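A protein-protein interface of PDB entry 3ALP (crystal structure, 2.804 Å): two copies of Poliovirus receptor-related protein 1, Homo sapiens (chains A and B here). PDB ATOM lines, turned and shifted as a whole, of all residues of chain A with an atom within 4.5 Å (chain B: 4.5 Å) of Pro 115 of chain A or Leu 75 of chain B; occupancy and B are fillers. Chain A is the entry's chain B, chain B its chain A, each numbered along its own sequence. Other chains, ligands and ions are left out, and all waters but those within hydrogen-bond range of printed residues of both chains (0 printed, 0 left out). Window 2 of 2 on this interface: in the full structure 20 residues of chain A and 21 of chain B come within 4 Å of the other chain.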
ATOM      1  N   SER A  44      -7.401   5.221  19.187  1.00  0.00           N
ATOM      2  CA  SER A  44      -7.816   3.914  18.680  1.00  0.00           C
ATOM      3  C   SER A  44      -7.962   2.852  19.780  1.00  0.00           C
ATOM      4  O   SER A  44      -8.989   2.170  19.856  1.00  0.00           O
ATOM      5  CB  SER A  44      -6.800   3.446  17.641  1.00  0.00           C
ATOM      6  OG  SER A  44      -6.110   4.563  17.100  1.00  0.00           O
ATOM      7  N   PHE A 114      -8.476  -3.060  23.778  1.00  0.00           N
ATOM      8  CA  PHE A 114      -9.149  -3.477  22.546  1.00  0.00           C
ATOM      9  C   PHE A 114      -9.056  -2.369  21.515  1.00  0.00           C
ATOM     10  O   PHE A 114      -9.189  -1.190  21.850  1.00  0.00           O
ATOM     11  CB  PHE A 114     -10.615  -3.800  22.811  1.00  0.00           C
ATOM     12  CG  PHE A 114     -11.336  -4.353  21.615  1.00  0.00           C
ATOM     13  CD1 PHE A 114     -11.556  -5.717  21.496  1.00  0.00           C
ATOM     14  CD2 PHE A 114     -11.797  -3.508  20.612  1.00  0.00           C
ATOM     15  CE1 PHE A 114     -12.213  -6.237  20.396  1.00  0.00           C
ATOM     16  CE2 PHE A 114     -12.457  -4.018  19.514  1.00  0.00           C
ATOM     17  CZ  PHE A 114     -12.667  -5.389  19.406  1.00  0.00           C
ATOM     18  N   PRO A 115      -8.836  -2.734  20.249  1.00  0.00           N
ATOM     19  CA  PRO A 115      -8.761  -4.087  19.702  1.00  0.00           C
ATOM     20  C   PRO A 115      -7.322  -4.564  19.655  1.00  0.00           C
ATOM     21  O   PRO A 115      -6.956  -5.484  18.916  1.00  0.00           O
ATOM     22  CB  PRO A 115      -9.211  -3.849  18.277  1.00  0.00           C
ATOM     23  CG  PRO A 115      -8.453  -2.591  17.933  1.00  0.00           C
ATOM     24  CD  PRO A 115      -8.502  -1.744  19.207  1.00  0.00           C
ATOM     25  N   THR A 116      -6.497  -3.922  20.456  1.00  0.00           N
ATOM     26  CA  THR A 116      -5.081  -4.011  20.232  1.00  0.00           C
ATOM     27  C   THR A 116      -4.410  -5.085  21.108  1.00  0.00           C
ATOM     28  O   THR A 116      -3.221  -5.379  20.930  1.00  0.00           O
ATOM     29  CB  THR A 116      -4.464  -2.614  20.384  1.00  0.00           C
ATOM     30  OG1 THR A 116      -3.489  -2.410  19.361  1.00  0.00           O
ATOM     31  CG2 THR A 116      -3.844  -2.432  21.742  1.00  0.00           C
ATOM     32  N   GLY A 117      -5.178  -5.687  22.021  1.00  0.00           N
ATOM     33  CA  GLY A 117      -4.654  -6.742  22.877  1.00  0.00           C
ATOM     34  C   GLY A 117      -4.067  -6.285  24.211  1.00  0.00           C
ATOM     35  O   GLY A 117      -4.285  -5.151  24.627  1.00  0.00           O
ATOM     36  N   ASN B  62       0.172 -10.574  20.872  1.00  0.00           N
ATOM     37  CA  ASN B  62      -1.273 -10.777  20.820  1.00  0.00           C
ATOM     38  C   ASN B  62      -1.728 -11.431  19.527  1.00  0.00           C
ATOM     39  O   ASN B  62      -1.201 -11.151  18.460  1.00  0.00           O
ATOM     40  CB  ASN B  62      -2.025  -9.481  21.091  1.00  0.00           C
ATOM     41  CG  ASN B  62      -1.696  -8.901  22.452  1.00  0.00           C
ATOM     42  OD1 ASN B  62      -2.277  -9.286  23.463  1.00  0.00           O
ATOM     43  ND2 ASN B  62      -0.746  -7.977  22.483  1.00  0.00           N
ATOM     44  N   VAL B  63      -2.694 -12.329  19.646  1.00  0.00           N
ATOM     45  CA  VAL B  63      -3.150 -13.130  18.524  1.00  0.00           C
ATOM     46  C   VAL B  63      -4.580 -12.780  18.125  1.00  0.00           C
ATOM     47  O   VAL B  63      -4.842 -12.394  16.987  1.00  0.00           O
ATOM     48  CB  VAL B  63      -3.101 -14.615  18.879  1.00  0.00           C
ATOM     49  CG1 VAL B  63      -3.740 -15.439  17.786  1.00  0.00           C
ATOM     50  CG2 VAL B  63      -1.673 -15.030  19.137  1.00  0.00           C
ATOM     51  N   ILE B  65      -8.549 -11.287  20.008  1.00  0.00           N
ATOM     52  CA  ILE B  65      -9.267 -10.740  21.158  1.00  0.00           C
ATOM     53  C   ILE B  65     -10.746 -10.804  20.876  1.00  0.00           C
ATOM     54  O   ILE B  65     -11.170 -10.529  19.763  1.00  0.00           O
ATOM     55  CB  ILE B  65      -8.949  -9.240  21.409  1.00  0.00           C
ATOM     56  CG1 ILE B  65      -7.473  -9.006  21.679  1.00  0.00           C
ATOM     57  CG2 ILE B  65      -9.702  -8.759  22.595  1.00  0.00           C
ATOM     58  CD1 ILE B  65      -6.625  -9.022  20.436  1.00  0.00           C
ATOM     59  N   SER B  73     -11.455  -9.105  17.335  1.00  0.00           N
ATOM     60  CA  SER B  73     -10.312  -8.506  16.670  1.00  0.00           C
ATOM     61  C   SER B  73      -9.215  -9.553  16.502  1.00  0.00           C
ATOM     62  O   SER B  73      -8.730 -10.129  17.470  1.00  0.00           O
ATOM     63  CB  SER B  73      -9.792  -7.320  17.482  1.00  0.00           C
ATOM     64  OG  SER B  73      -8.425  -7.044  17.205  1.00  0.00           O
ATOM     65  N   VAL B  74      -8.838  -9.828  15.262  1.00  0.00           N
ATOM     66  CA  VAL B  74      -7.702 -10.694  15.024  1.00  0.00           C
ATOM     67  C   VAL B  74      -6.577  -9.799  14.567  1.00  0.00           C
ATOM     68  O   VAL B  74      -6.792  -8.845  13.831  1.00  0.00           O
ATOM     69  CB  VAL B  74      -7.996 -11.778  13.971  1.00  0.00           C
ATOM     70  CG1 VAL B  74      -6.810 -12.734  13.844  1.00  0.00           C
ATOM     71  CG2 VAL B  74      -9.271 -12.538  14.326  1.00  0.00           C
ATOM     72  N   LEU B  75      -5.374 -10.091  15.026  1.00  0.00           N
ATOM     73  CA  LEU B  75      -4.254  -9.217  14.769  1.00  0.00           C
ATOM     74  C   LEU B  75      -3.325  -9.823  13.746  1.00  0.00           C
ATOM     75  O   LEU B  75      -3.215 -11.042  13.629  1.00  0.00           O
ATOM     76  CB  LEU B  75      -3.481  -8.993  16.057  1.00  0.00           C
ATOM     77  CG  LEU B  75      -4.286  -8.373  17.186  1.00  0.00           C
ATOM     78  CD1 LEU B  75      -3.423  -8.285  18.404  1.00  0.00           C
ATOM     79  CD2 LEU B  75      -4.752  -7.001  16.791  1.00  0.00           C
ATOM     80  N   ALA B  76      -2.649  -8.962  12.999  1.00  0.00           N
ATOM     81  CA  ALA B  76      -1.588  -9.428  12.135  1.00  0.00           C
ATOM     82  C   ALA B  76      -0.575 -10.171  12.990  1.00  0.00           C
ATOM     83  O   ALA B  76      -0.318  -9.788  14.136  1.00  0.00           O
ATOM     84  CB  ALA B  76      -0.944  -8.264  11.442  1.00  0.00           C
ATOM     85  N   PRO B  77       0.019 -11.234  12.440  1.00  0.00           N
ATOM     86  CA  PRO B  77      -0.133 -11.790  11.090  1.00  0.00           C
ATOM     87  C   PRO B  77      -1.113 -12.947  11.018  1.00  0.00           C
ATOM     88  O   PRO B  77      -0.760 -14.012  10.513  1.00  0.00           O
ATOM     89  CB  PRO B  77       1.256 -12.369  10.804  1.00  0.00           C
ATOM     90  CG  PRO B  77       2.039 -12.275  12.100  1.00  0.00           C
ATOM     91  CD  PRO B  77       1.086 -11.917  13.180  1.00  0.00           C
ATOM     92  N   TYR B  78      -2.320 -12.759  11.517  1.00  0.00           N
ATOM     93  CA  TYR B  78      -3.232 -13.877  11.649  1.00  0.00           C
ATOM     94  C   TYR B  78      -4.586 -13.594  11.035  1.00  0.00           C
ATOM     95  O   TYR B  78      -5.504 -14.389  11.211  1.00  0.00           O
ATOM     96  CB  TYR B  78      -3.463 -14.183  13.128  1.00  0.00           C
ATOM     97  CG  TYR B  78      -2.260 -14.702  13.879  1.00  0.00           C
ATOM     98  CD1 TYR B  78      -1.773 -15.975  13.638  1.00  0.00           C
ATOM     99  CD2 TYR B  78      -1.631 -13.935  14.859  1.00  0.00           C
ATOM    100  CE1 TYR B  78      -0.689 -16.468  14.329  1.00  0.00           C
ATOM    101  CE2 TYR B  78      -0.531 -14.424  15.553  1.00  0.00           C
ATOM    102  CZ  TYR B  78      -0.070 -15.694  15.279  1.00  0.00           C
ATOM    103  OH  TYR B  78       1.017 -16.212  15.935  1.00  0.00           O
ATOM    104  N   ARG B  79      -4.739 -12.463  10.346  1.00  0.00           N
ATOM    105  CA  ARG B  79      -6.094 -12.009  10.027  1.00  0.00           C
ATOM    106  C   ARG B  79      -6.781 -13.083   9.205  1.00  0.00           C
ATOM    107  O   ARG B  79      -7.992 -13.291   9.313  1.00  0.00           O
ATOM    108  CB  ARG B  79      -6.144 -10.648   9.299  1.00  0.00           C
ATOM    109  CG  ARG B  79      -5.449  -9.489   9.995  1.00  0.00           C
ATOM    110  CD  ARG B  79      -4.031  -9.286   9.438  1.00  0.00           C
ATOM    111  NE  ARG B  79      -3.335 -10.553   9.191  1.00  0.00           N
ATOM    112  CZ  ARG B  79      -2.167 -10.669   8.565  1.00  0.00           C
ATOM    113  NH1 ARG B  79      -1.538  -9.594   8.107  1.00  0.00           N
ATOM    114  NH2 ARG B  79      -1.627 -11.868   8.396  1.00  0.00           N
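The backbone carbonyl oxygen of Pro 115 of chain A is in hydrogen-bond range of the side-chain hydroxyl of Ser 73 of chain B (2.7 Å).
The backbone NH (N) of Ile 65 of chain B sits at hydrogen-bond distance from the backbone carbonyl oxygen (O) of Ser 73 of chain B (2.8 Å).
The backbone carbonyl oxygen of Val 63 of chain B sits at hydrogen-bond distance from the backbone NH of Leu 75 of chain B, at 3.1 Å.
Phe 114 of chain A touches Ile 65 of chain B.
CB of Ser 73 of chain B touches CE1 of Phe 114 of chain A (3.9 Å).
CD1 of Ile 65 of chain B touches O of Pro 115 of chain A (3.9 Å).
Leu 75 of chain B touches Pro 115 of chain A.
Asn 62 of chain B touches Thr 116 of chain A.
Leu 75 of chain B touches Thr 116 of chain A (CD1 to O, 3.9 Å).
CA of Gly 117 of chain A touches OD1 of Asn 62 of chain B (3.5 Å).
Gly 117 of chain A touches Ile 65 of chain B (CA to CG1, 3.8 Å).
Pro 115 of chain A touches just these residues of chain B: Ile 65 (3.9 Å), Ser 73 (2.7 Å) and Leu 75 (3.4 Å).
Leu 75 of chain B touches two residues of chain A.
Printed residues of chain B within 4 Å of Gly 117 of chain A: Asn 62 and Ile 65.
Of the printed residues of chain A, Ser 73 of chain B touches Phe 114 (3.9 Å) and Pro 115 (2.7 Å).
Of the printed residues of chain A, Ile 65 of chain B touches Phe 114, Pro 115 and Gly 117.
The nearest printed residue of chain B that does not touch Pro 115 of chain A is Val 74 of chain B (6.0 Å).
The nearest printed residue of chain A that does not touch Leu 75 of chain B is Gly 117 of chain A (4.8 Å).
The nearest printed residue of chain A that does not touch Ile 65 of chain B is Thr 116 of chain A (4.6 Å).
Hydrophobic or aromatic side chains of chain B within 4 Å of the printed part of chain A: Ile 65 and Leu 75.
Of the 5 printed residues of chain A, 4 touch a printed residue of chain B.
Printed residues of chain A that touch a printed residue of chain B: Phe 114, Pro 115, Thr 116 and Gly 117.
Hydrophobic or aromatic side chains of chain A within 4 Å of the printed part of chain B: Phe 114 and Pro 115.
No position is printed for both chains.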
